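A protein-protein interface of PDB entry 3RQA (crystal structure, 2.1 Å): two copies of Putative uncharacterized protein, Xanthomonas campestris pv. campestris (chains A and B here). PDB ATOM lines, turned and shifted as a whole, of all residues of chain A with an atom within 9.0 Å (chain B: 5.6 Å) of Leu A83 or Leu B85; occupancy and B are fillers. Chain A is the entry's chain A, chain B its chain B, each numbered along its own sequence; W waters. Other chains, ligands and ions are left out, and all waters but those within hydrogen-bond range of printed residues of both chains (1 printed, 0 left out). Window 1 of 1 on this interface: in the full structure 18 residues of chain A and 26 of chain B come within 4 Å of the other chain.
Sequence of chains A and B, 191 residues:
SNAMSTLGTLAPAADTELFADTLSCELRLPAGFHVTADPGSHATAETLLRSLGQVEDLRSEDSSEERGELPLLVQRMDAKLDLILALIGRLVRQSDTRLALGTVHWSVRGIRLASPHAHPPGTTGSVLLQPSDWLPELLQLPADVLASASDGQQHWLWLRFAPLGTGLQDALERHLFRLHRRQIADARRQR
Printed residues of chain A that touch a printed residue of chain B: Arg A76, Met A77, Ala A79, Lys A80, Leu A81, Asp A82, Leu A83, Ile A84, Ala A86, Leu A87, Ile A88, Arg A90 and Leu A91.
Hydrophobic or aromatic side chains of chain A within 4 Å of the printed part of chain B: Met A77, Ala A79, Leu A81, Leu A83, Ile A84, Ala A86, Leu A87, Ile A88 and Leu A91.
Hydrophobic or aromatic side chains of chain B within 4 Å of the printed part of chain A: Leu B52, Val B55, Leu B81, Ile B84, Leu B85, Ile B88 and Leu B135.
Among the printed residues, 22 pairs touch across the chains.
Among the printed residues, Asp or Glu carboxylates within 4 Å of a Lys or Arg side-chain nitrogen of the other chain: Lys A80 with Asp B82 (3.0 Å) and Arg A90 with Glu B137 (2.7 Å).
OD1 of Asp B82 is in salt-bridge range of NZ of Lys A80 (3.0 Å).
OD1 of Asp A82 sits at hydrogen-bond distance from OG of Ser B51, at 3.3 Å.
The guanidinium group of Arg A90 lies within salt-bridge range of the side-chain carboxylate of Glu B137 (2.7 Å).
Leu A83 touches just these residues of chain B: Ser B51 (3.9 Å), Leu B52 (3.4 Å), Leu B85 (3.8 Å) and Leu B135 (3.3 Å).
Leu B85 touches three residues of chain A.
No residue of chain A comes within 4 Å of Ala B86.
Of the printed residues of chain A, Leu B52 touches Leu A83.
Of the printed residues of chain A, Ile B88 touches Leu A87, Ile A88 and Leu A91.
Of the printed residues of chain B, Leu A81 touches Leu B81.
Printed residues of chain B within 4 Å of Asp A82: Ser B51 (3.3 Å).
Of the printed residues of chain A, Leu B81 touches Met A77, Leu A81 and Ile A84.
Leu B83 touches none of the printed residues of chain A.
The nearest residue of chain B that does not touch Leu A83 is Leu B48 (4.1 Å).
Lys A80 touches Asp B82, but with the chains exchanged Asp A82 does not touch Lys B80 (11.9 Å).
Leu A81 touches its own counterpart, Leu B81.
Leu A83 touches Leu B85, but with the chains exchanged Leu A85 does not touch Leu B83 (11.4 Å).
Leu A87 touches Leu B85, but with the chains exchanged Leu A85 does not touch Leu B87 (10.8 Å).
Positions printed for both chains: 80, 81, 82, 83, 84, 85, 86, 87, 88, 89 and 90.
Of the 22 pairs that touch across the chains among the printed residues, 3 have their exchanged pair printed and touching as well.
CB of Met A77 touches CD1 of Leu B81, at 3.5 Å.
Ala A79 touches Val B55.
Ser B51 touches Leu A83 (CB to CD2, 3.9 Å).
CD2 of Leu A83 touches CD2 of Leu B135 (3.3 Å).
CD1 of Ile A84 touches CD2 of Leu B81, at 3.7 Å.
CG2 of Ile B84 touches CG2 of Ile A84, 3.7 Å away.
Ala A86 touches Glu B137 (CB to OE1, 3.7 Å).
Leu A87 touches Ile B88.
OE2 of Glu B137 touches N of Leu A87 (3.8 Å).
Ile A88 touches Ile B88.
Water W1 bridges OE1 of Glu B137 (2.7 Å) and O of Ala A86 (2.9 Å).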
ATOM      1  N   ARG A  76      23.625   1.853 -30.792  1.00  0.00           N
ATOM      2  CA  ARG A  76      22.550   2.562 -30.131  1.00  0.00           C
ATOM      3  C   ARG A  76      22.238   1.978 -28.727  1.00  0.00           C
ATOM      4  O   ARG A  76      21.927   2.731 -27.796  1.00  0.00           O
ATOM      5  CB  ARG A  76      21.325   2.542 -31.060  1.00  0.00           C
ATOM      6  CG  ARG A  76      19.982   2.794 -30.406  1.00  0.00           C
ATOM      7  CD  ARG A  76      18.810   2.647 -31.431  1.00  0.00           C
ATOM      8  NE  ARG A  76      18.483   3.919 -32.081  1.00  0.00           N
ATOM      9  CZ  ARG A  76      19.283   4.533 -32.947  1.00  0.00           C
ATOM     10  NH1 ARG A  76      20.448   3.979 -33.262  1.00  0.00           N
ATOM     11  NH2 ARG A  76      18.935   5.707 -33.483  1.00  0.00           N
ATOM     12  N   MET A  77      22.330   0.654 -28.578  1.00  0.00           N
ATOM     13  CA  MET A  77      22.100   0.031 -27.268  1.00  0.00           C
ATOM     14  C   MET A  77      23.229   0.490 -26.340  1.00  0.00           C
ATOM     15  O   MET A  77      22.992   0.791 -25.167  1.00  0.00           O
ATOM     16  CB  MET A  77      22.110  -1.505 -27.365  1.00  0.00           C
ATOM     17  CG  MET A  77      20.884  -2.117 -28.057  1.00  0.00           C
ATOM     18  SD  MET A  77      21.069  -3.872 -28.501  1.00  0.00           S
ATOM     19  CE  MET A  77      20.492  -4.609 -27.074  1.00  0.00           C
ATOM     20  N   ASP A  78      24.454   0.537 -26.866  1.00  0.00           N
ATOM     21  CA  ASP A  78      25.611   0.979 -26.084  1.00  0.00           C
ATOM     22  C   ASP A  78      25.374   2.394 -25.558  1.00  0.00           C
ATOM     23  O   ASP A  78      25.698   2.713 -24.406  1.00  0.00           O
ATOM     24  CB  ASP A  78      26.881   0.964 -26.935  1.00  0.00           C
ATOM     25  CG  ASP A  78      28.085   1.546 -26.198  1.00  0.00           C
ATOM     26  OD1 ASP A  78      28.486   0.995 -25.145  1.00  0.00           O
ATOM     27  OD2 ASP A  78      28.627   2.567 -26.672  1.00  0.00           O
ATOM     28  N   ALA A  79      24.806   3.242 -26.410  1.00  0.00           N
ATOM     29  CA  ALA A  79      24.507   4.615 -26.034  1.00  0.00           C
ATOM     30  C   ALA A  79      23.545   4.607 -24.855  1.00  0.00           C
ATOM     31  O   ALA A  79      23.766   5.295 -23.855  1.00  0.00           O
ATOM     32  CB  ALA A  79      23.892   5.353 -27.210  1.00  0.00           C
ATOM     33  N   LYS A  80      22.481   3.814 -24.972  1.00  0.00           N
ATOM     34  CA  LYS A  80      21.487   3.715 -23.906  1.00  0.00           C
ATOM     35  C   LYS A  80      22.153   3.316 -22.590  1.00  0.00           C
ATOM     36  O   LYS A  80      21.736   3.760 -21.520  1.00  0.00           O
ATOM     37  CB  LYS A  80      20.400   2.697 -24.279  1.00  0.00           C
ATOM     38  CG  LYS A  80      19.591   3.093 -25.495  1.00  0.00           C
ATOM     39  CD  LYS A  80      18.535   2.064 -25.835  1.00  0.00           C
ATOM     40  CE  LYS A  80      17.962   2.349 -27.233  1.00  0.00           C
ATOM     41  NZ  LYS A  80      16.957   1.383 -27.725  1.00  0.00           N
ATOM     42  N   LEU A  81      23.180   2.470 -22.678  1.00  0.00           N
ATOM     43  CA  LEU A  81      23.920   2.043 -21.498  1.00  0.00           C
ATOM     44  C   LEU A  81      24.614   3.237 -20.860  1.00  0.00           C
ATOM     45  O   LEU A  81      24.574   3.396 -19.642  1.00  0.00           O
ATOM     46  CB  LEU A  81      24.957   0.967 -21.860  1.00  0.00           C
ATOM     47  CG  LEU A  81      24.422  -0.466 -22.017  1.00  0.00           C
ATOM     48  CD1 LEU A  81      25.552  -1.388 -22.455  1.00  0.00           C
ATOM     49  CD2 LEU A  81      23.801  -0.949 -20.695  1.00  0.00           C
ATOM     50  N   ASP A  82      25.239   4.076 -21.690  1.00  0.00           N
ATOM     51  CA  ASP A  82      25.927   5.271 -21.203  1.00  0.00           C
ATOM     52  C   ASP A  82      24.933   6.151 -20.464  1.00  0.00           C
ATOM     53  O   ASP A  82      25.230   6.680 -19.393  1.00  0.00           O
ATOM     54  CB  ASP A  82      26.531   6.060 -22.368  1.00  0.00           C
ATOM     55  CG  ASP A  82      27.802   5.433 -22.899  1.00  0.00           C
ATOM     56  OD1 ASP A  82      28.185   5.745 -24.047  1.00  0.00           O
ATOM     57  OD2 ASP A  82      28.431   4.637 -22.172  1.00  0.00           O
ATOM     58  N   LEU A  83      23.748   6.297 -21.043  1.00  0.00           N
ATOM     59  CA  LEU A  83      22.701   7.104 -20.433  1.00  0.00           C
ATOM     60  C   LEU A  83      22.241   6.526 -19.089  1.00  0.00           C
ATOM     61  O   LEU A  83      22.147   7.246 -18.106  1.00  0.00           O
ATOM     62  CB  LEU A  83      21.521   7.225 -21.407  1.00  0.00           C
ATOM     63  CG  LEU A  83      21.877   7.987 -22.690  1.00  0.00           C
ATOM     64  CD1 LEU A  83      20.735   7.917 -23.703  1.00  0.00           C
ATOM     65  CD2 LEU A  83      22.198   9.435 -22.332  1.00  0.00           C
ATOM     66  N   ILE A  84      21.975   5.220 -19.046  1.00  0.00           N
ATOM     67  CA  ILE A  84      21.522   4.569 -17.813  1.00  0.00           C
ATOM     68  C   ILE A  84      22.553   4.728 -16.699  1.00  0.00           C
ATOM     69  O   ILE A  84      22.214   5.082 -15.576  1.00  0.00           O
ATOM     70  CB  ILE A  84      21.241   3.053 -18.053  1.00  0.00           C
ATOM     71  CG1 ILE A  84      19.998   2.895 -18.935  1.00  0.00           C
ATOM     72  CG2 ILE A  84      21.018   2.312 -16.725  1.00  0.00           C
ATOM     73  CD1 ILE A  84      20.076   1.688 -19.862  1.00  0.00           C
ATOM     74  N   LEU A  85      23.815   4.482 -17.023  1.00  0.00           N
ATOM     75  CA  LEU A  85      24.877   4.600 -16.038  1.00  0.00           C
ATOM     76  C   LEU A  85      24.929   6.024 -15.492  1.00  0.00           C
ATOM     77  O   LEU A  85      25.002   6.231 -14.282  1.00  0.00           O
ATOM     78  CB  LEU A  85      26.219   4.231 -16.682  1.00  0.00           C
ATOM     79  CG  LEU A  85      27.474   4.206 -15.813  1.00  0.00           C
ATOM     80  CD1 LEU A  85      27.308   3.251 -14.633  1.00  0.00           C
ATOM     81  CD2 LEU A  85      28.662   3.785 -16.692  1.00  0.00           C
ATOM     82  N   ALA A  86      24.868   7.008 -16.384  1.00  0.00           N
ATOM     83  CA  ALA A  86      24.923   8.395 -15.952  1.00  0.00           C
ATOM     84  C   ALA A  86      23.746   8.712 -15.043  1.00  0.00           C
ATOM     85  O   ALA A  86      23.929   9.241 -13.948  1.00  0.00           O
ATOM     86  CB  ALA A  86      24.932   9.341 -17.163  1.00  0.00           C
ATOM     87  N   LEU A  87      22.540   8.378 -15.496  1.00  0.00           N
ATOM     88  CA  LEU A  87      21.331   8.629 -14.714  1.00  0.00           C
ATOM     89  C   LEU A  87      21.373   7.971 -13.334  1.00  0.00           C
ATOM     90  O   LEU A  87      21.132   8.626 -12.323  1.00  0.00           O
ATOM     91  CB  LEU A  87      20.097   8.163 -15.501  1.00  0.00           C
ATOM     92  CG  LEU A  87      19.693   9.126 -16.632  1.00  0.00           C
ATOM     93  CD1 LEU A  87      18.764   8.440 -17.607  1.00  0.00           C
ATOM     94  CD2 LEU A  87      19.032  10.360 -16.030  1.00  0.00           C
ATOM     95  N   ILE A  88      21.695   6.684 -13.282  1.00  0.00           N
ATOM     96  CA  ILE A  88      21.756   6.004 -11.999  1.00  0.00           C
ATOM     97  C   ILE A  88      22.844   6.649 -11.143  1.00  0.00           C
ATOM     98  O   ILE A  88      22.725   6.725  -9.926  1.00  0.00           O
ATOM     99  CB  ILE A  88      22.022   4.493 -12.161  1.00  0.00           C
ATOM    100  CG1 ILE A  88      22.075   3.838 -10.788  1.00  0.00           C
ATOM    101  CG2 ILE A  88      23.327   4.258 -12.894  1.00  0.00           C
ATOM    102  CD1 ILE A  88      22.195   2.340 -10.850  1.00  0.00           C
ATOM    103  N   GLY A  89      23.894   7.138 -11.791  1.00  0.00           N
ATOM    104  CA  GLY A  89      24.956   7.799 -11.050  1.00  0.00           C
ATOM    105  C   GLY A  89      24.416   9.045 -10.369  1.00  0.00           C
ATOM    106  O   GLY A  89      24.660   9.290  -9.189  1.00  0.00           O
ATOM    107  N   ARG A  90      23.662   9.835 -11.123  1.00  0.00           N
ATOM    108  CA  ARG A  90      23.069  11.061 -10.601  1.00  0.00           C
ATOM    109  C   ARG A  90      22.144  10.774  -9.415  1.00  0.00           C
ATOM    110  O   ARG A  90      22.173  11.492  -8.413  1.00  0.00           O
ATOM    111  CB  ARG A  90      22.280  11.768 -11.703  1.00  0.00           C
ATOM    112  CG  ARG A  90      21.747  13.136 -11.316  1.00  0.00           C
ATOM    113  CD  ARG A  90      21.084  13.803 -12.506  1.00  0.00           C
ATOM    114  NE  ARG A  90      22.025  13.986 -13.610  1.00  0.00           N
ATOM    115  CZ  ARG A  90      23.014  14.877 -13.618  1.00  0.00           C
ATOM    116  NH1 ARG A  90      23.823  14.963 -14.669  1.00  0.00           N
ATOM    117  NH2 ARG A  90      23.189  15.695 -12.588  1.00  0.00           N
ATOM    118  N   LEU A  91      21.334   9.718  -9.539  1.00  0.00           N
ATOM    119  CA  LEU A  91      20.384   9.316  -8.499  1.00  0.00           C
ATOM    120  C   LEU A  91      21.117   8.945  -7.219  1.00  0.00           C
ATOM    121  O   LEU A  91      20.715   9.342  -6.122  1.00  0.00           O
ATOM    122  CB  LEU A  91      19.557   8.119  -8.979  1.00  0.00           C
ATOM    123  CG  LEU A  91      18.152   7.920  -8.400  1.00  0.00           C
ATOM    124  CD1 LEU A  91      17.529   6.659  -9.006  1.00  0.00           C
ATOM    125  CD2 LEU A  91      18.219   7.808  -6.885  1.00  0.00           C
ATOM    126  N   LEU B  48      27.752  12.112 -22.866  1.00  0.00           N
ATOM    127  CA  LEU B  48      26.356  12.506 -22.765  1.00  0.00           C
ATOM    128  C   LEU B  48      25.800  13.021 -24.092  1.00  0.00           C
ATOM    129  O   LEU B  48      24.724  12.599 -24.531  1.00  0.00           O
ATOM    130  CB  LEU B  48      26.178  13.569 -21.676  1.00  0.00           C
ATOM    131  CG  LEU B  48      24.773  14.174 -21.566  1.00  0.00           C
ATOM    132  CD1 LEU B  48      23.740  13.073 -21.340  1.00  0.00           C
ATOM    133  CD2 LEU B  48      24.745  15.197 -20.442  1.00  0.00           C
ATOM    134  N   SER B  51      25.735  10.250 -26.920  1.00  0.00           N
ATOM    135  CA  SER B  51      24.736   9.248 -26.597  1.00  0.00           C
ATOM    136  C   SER B  51      23.323   9.734 -26.871  1.00  0.00           C
ATOM    137  O   SER B  51      22.486   8.977 -27.372  1.00  0.00           O
ATOM    138  CB  SER B  51      24.885   8.802 -25.148  1.00  0.00           C
ATOM    139  OG  SER B  51      25.981   7.921 -25.050  1.00  0.00           O
ATOM    140  N   LEU B  52      23.052  10.991 -26.540  1.00  0.00           N
ATOM    141  CA  LEU B  52      21.738  11.556 -26.805  1.00  0.00           C
ATOM    142  C   LEU B  52      21.512  11.510 -28.307  1.00  0.00           C
ATOM    143  O   LEU B  52      20.421  11.216 -28.780  1.00  0.00           O
ATOM    144  CB  LEU B  52      21.675  13.008 -26.342  1.00  0.00           C
ATOM    145  CG  LEU B  52      21.131  13.280 -24.944  1.00  0.00           C
ATOM    146  CD1 LEU B  52      21.883  12.458 -23.922  1.00  0.00           C
ATOM    147  CD2 LEU B  52      21.265  14.755 -24.645  1.00  0.00           C
ATOM    148  N   VAL B  55      20.952   7.814 -30.047  1.00  0.00           N
ATOM    149  CA  VAL B  55      19.625   7.257 -29.835  1.00  0.00           C
ATOM    150  C   VAL B  55      18.625   8.154 -30.563  1.00  0.00           C
ATOM    151  O   VAL B  55      17.537   8.434 -30.063  1.00  0.00           O
ATOM    152  CB  VAL B  55      19.280   7.179 -28.321  1.00  0.00           C
ATOM    153  CG1 VAL B  55      20.393   6.454 -27.577  1.00  0.00           C
ATOM    154  CG2 VAL B  55      19.091   8.556 -27.746  1.00  0.00           C
ATOM    155  N   LYS B  80      14.526  -4.316 -22.985  1.00  0.00           N
ATOM    156  CA  LYS B  80      14.856  -4.257 -21.572  1.00  0.00           C
ATOM    157  C   LYS B  80      15.575  -2.952 -21.255  1.00  0.00           C
ATOM    158  O   LYS B  80      15.286  -2.308 -20.249  1.00  0.00           O
ATOM    159  CB  LYS B  80      15.723  -5.451 -21.189  1.00  0.00           C
ATOM    160  CG  LYS B  80      14.955  -6.763 -21.237  1.00  0.00           C
ATOM    161  CD  LYS B  80      15.797  -7.974 -20.902  1.00  0.00           C
ATOM    162  CE  LYS B  80      14.985  -9.248 -21.140  1.00  0.00           C
ATOM    163  NZ  LYS B  80      15.753 -10.489 -20.925  1.00  0.00           N
ATOM    164  N   LEU B  81      16.512  -2.569 -22.118  1.00  0.00           N
ATOM    165  CA  LEU B  81      17.246  -1.320 -21.944  1.00  0.00           C
ATOM    166  C   LEU B  81      16.263  -0.141 -21.936  1.00  0.00           C
ATOM    167  O   LEU B  81      16.339   0.733 -21.065  1.00  0.00           O
ATOM    168  CB  LEU B  81      18.266  -1.139 -23.075  1.00  0.00           C
ATOM    169  CG  LEU B  81      19.585  -1.928 -23.014  1.00  0.00           C
ATOM    170  CD1 LEU B  81      20.357  -1.719 -24.310  1.00  0.00           C
ATOM    171  CD2 LEU B  81      20.419  -1.481 -21.825  1.00  0.00           C
ATOM    172  N   ASP B  82      15.336  -0.123 -22.895  1.00  0.00           N
ATOM    173  CA  ASP B  82      14.356   0.955 -22.952  1.00  0.00           C
ATOM    174  C   ASP B  82      13.591   1.059 -21.639  1.00  0.00           C
ATOM    175  O   ASP B  82      13.396   2.152 -21.129  1.00  0.00           O
ATOM    176  CB  ASP B  82      13.366   0.753 -24.105  1.00  0.00           C
ATOM    177  CG  ASP B  82      14.008   0.954 -25.471  1.00  0.00           C
ATOM    178  OD1 ASP B  82      14.961   1.761 -25.578  1.00  0.00           O
ATOM    179  OD2 ASP B  82      13.550   0.317 -26.438  1.00  0.00           O
ATOM    180  N   LEU B  83      13.167  -0.079 -21.092  1.00  0.00           N
ATOM    181  CA  LEU B  83      12.428  -0.096 -19.827  1.00  0.00           C
ATOM    182  C   LEU B  83      13.267   0.457 -18.672  1.00  0.00           C
ATOM    183  O   LEU B  83      12.771   1.227 -17.857  1.00  0.00           O
ATOM    184  CB  LEU B  83      11.976  -1.525 -19.497  1.00  0.00           C
ATOM    185  CG  LEU B  83      10.509  -1.973 -19.614  1.00  0.00           C
ATOM    186  CD1 LEU B  83       9.642  -0.928 -20.294  1.00  0.00           C
ATOM    187  CD2 LEU B  83      10.461  -3.297 -20.377  1.00  0.00           C
ATOM    188  N   ILE B  84      14.535   0.053 -18.608  1.00  0.00           N
ATOM    189  CA  ILE B  84      15.455   0.504 -17.568  1.00  0.00           C
ATOM    190  C   ILE B  84      15.680   2.019 -17.636  1.00  0.00           C
ATOM    191  O   ILE B  84      15.608   2.725 -16.627  1.00  0.00           O
ATOM    192  CB  ILE B  84      16.836  -0.172 -17.716  1.00  0.00           C
ATOM    193  CG1 ILE B  84      16.715  -1.685 -17.496  1.00  0.00           C
ATOM    194  CG2 ILE B  84      17.832   0.465 -16.748  1.00  0.00           C
ATOM    195  CD1 ILE B  84      18.043  -2.423 -17.606  1.00  0.00           C
ATOM    196  N   LEU B  85      15.974   2.502 -18.840  1.00  0.00           N
ATOM    197  CA  LEU B  85      16.222   3.918 -19.056  1.00  0.00           C
ATOM    198  C   LEU B  85      14.979   4.711 -18.669  1.00  0.00           C
ATOM    199  O   LEU B  85      15.063   5.714 -17.960  1.00  0.00           O
ATOM    200  CB  LEU B  85      16.570   4.169 -20.525  1.00  0.00           C
ATOM    201  CG  LEU B  85      17.047   5.560 -20.933  1.00  0.00           C
ATOM    202  CD1 LEU B  85      18.172   6.045 -20.041  1.00  0.00           C
ATOM    203  CD2 LEU B  85      17.532   5.478 -22.350  1.00  0.00           C
ATOM    204  N   ALA B  86      13.821   4.248 -19.127  1.00  0.00           N
ATOM    205  CA  ALA B  86      12.583   4.938 -18.814  1.00  0.00           C
ATOM    206  C   ALA B  86      12.355   5.044 -17.304  1.00  0.00           C
ATOM    207  O   ALA B  86      12.061   6.122 -16.797  1.00  0.00           O
ATOM    208  CB  ALA B  86      11.405   4.235 -19.488  1.00  0.00           C
ATOM    209  N   LEU B  87      12.502   3.933 -16.586  1.00  0.00           N
ATOM    210  CA  LEU B  87      12.301   3.938 -15.142  1.00  0.00           C
ATOM    211  C   LEU B  87      13.335   4.807 -14.423  1.00  0.00           C
ATOM    212  O   LEU B  87      12.986   5.642 -13.581  1.00  0.00           O
ATOM    213  CB  LEU B  87      12.349   2.506 -14.584  1.00  0.00           C
ATOM    214  CG  LEU B  87      11.055   1.675 -14.520  1.00  0.00           C
ATOM    215  CD1 LEU B  87      11.359   0.199 -14.715  1.00  0.00           C
ATOM    216  CD2 LEU B  87      10.374   1.880 -13.167  1.00  0.00           C
ATOM    217  N   ILE B  88      14.606   4.616 -14.756  1.00  0.00           N
ATOM    218  CA  ILE B  88      15.650   5.381 -14.106  1.00  0.00           C
ATOM    219  C   ILE B  88      15.488   6.872 -14.417  1.00  0.00           C
ATOM    220  O   ILE B  88      15.666   7.720 -13.547  1.00  0.00           O
ATOM    221  CB  ILE B  88      17.067   4.882 -14.537  1.00  0.00           C
ATOM    222  CG1 ILE B  88      18.116   5.423 -13.576  1.00  0.00           C
ATOM    223  CG2 ILE B  88      17.404   5.341 -15.946  1.00  0.00           C
ATOM    224  CD1 ILE B  88      18.053   4.802 -12.209  1.00  0.00           C
ATOM    225  N   GLY B  89      15.130   7.186 -15.656  1.00  0.00           N
ATOM    226  CA  GLY B  89      14.957   8.578 -16.025  1.00  0.00           C
ATOM    227  C   GLY B  89      13.914   9.263 -15.161  1.00  0.00           C
ATOM    228  O   GLY B  89      14.136  10.370 -14.653  1.00  0.00           O
ATOM    229  N   ARG B  90      12.776   8.592 -14.990  1.00  0.00           N
ATOM    230  CA  ARG B  90      11.673   9.115 -14.195  1.00  0.00           C
ATOM    231  C   ARG B  90      12.052   9.338 -12.732  1.00  0.00           C
ATOM    232  O   ARG B  90      11.682  10.360 -12.149  1.00  0.00           O
ATOM    233  CB  ARG B  90      10.467   8.172 -14.278  1.00  0.00           C
ATOM    234  CG  ARG B  90       9.304   8.567 -13.378  1.00  0.00           C
ATOM    235  CD  ARG B  90       8.053   7.754 -13.692  1.00  0.00           C
ATOM    236  NE  ARG B  90       8.123   6.367 -13.236  1.00  0.00           N
ATOM    237  CZ  ARG B  90       8.198   6.001 -11.959  1.00  0.00           C
ATOM    238  NH1 ARG B  90       8.255   4.718 -11.634  1.00  0.00           N
ATOM    239  NH2 ARG B  90       8.228   6.919 -11.006  1.00  0.00           N
ATOM    240  N   LEU B 135      14.979  13.090 -21.160  1.00  0.00           N
ATOM    241  CA  LEU B 135      16.067  12.567 -20.350  1.00  0.00           C
ATOM    242  C   LEU B 135      16.487  13.686 -19.401  1.00  0.00           C
ATOM    243  O   LEU B 135      16.825  14.788 -19.834  1.00  0.00           O
ATOM    244  CB  LEU B 135      17.227  12.158 -21.263  1.00  0.00           C
ATOM    245  CG  LEU B 135      18.239  11.115 -20.783  1.00  0.00           C
ATOM    246  CD1 LEU B 135      17.537   9.802 -20.497  1.00  0.00           C
ATOM    247  CD2 LEU B 135      19.300  10.921 -21.858  1.00  0.00           C
ATOM    248  N   GLU B 137      19.175  13.985 -17.660  1.00  0.00           N
ATOM    249  CA  GLU B 137      20.615  14.047 -17.430  1.00  0.00           C
ATOM    250  C   GLU B 137      21.139  15.433 -17.774  1.00  0.00           C
ATOM    251  O   GLU B 137      20.879  15.951 -18.860  1.00  0.00           O
ATOM    252  CB  GLU B 137      21.349  13.000 -18.266  1.00  0.00           C
ATOM    253  CG  GLU B 137      22.862  13.022 -18.064  1.00  0.00           C
ATOM    254  CD  GLU B 137      23.278  12.680 -16.646  1.00  0.00           C
ATOM    255  OE1 GLU B 137      24.452  12.939 -16.296  1.00  0.00           O
ATOM    256  OE2 GLU B 137      22.439  12.144 -15.887  1.00  0.00           O
HETATM  257  O   HOH W   1      25.319  11.798 -13.975  1.00  0.00           O
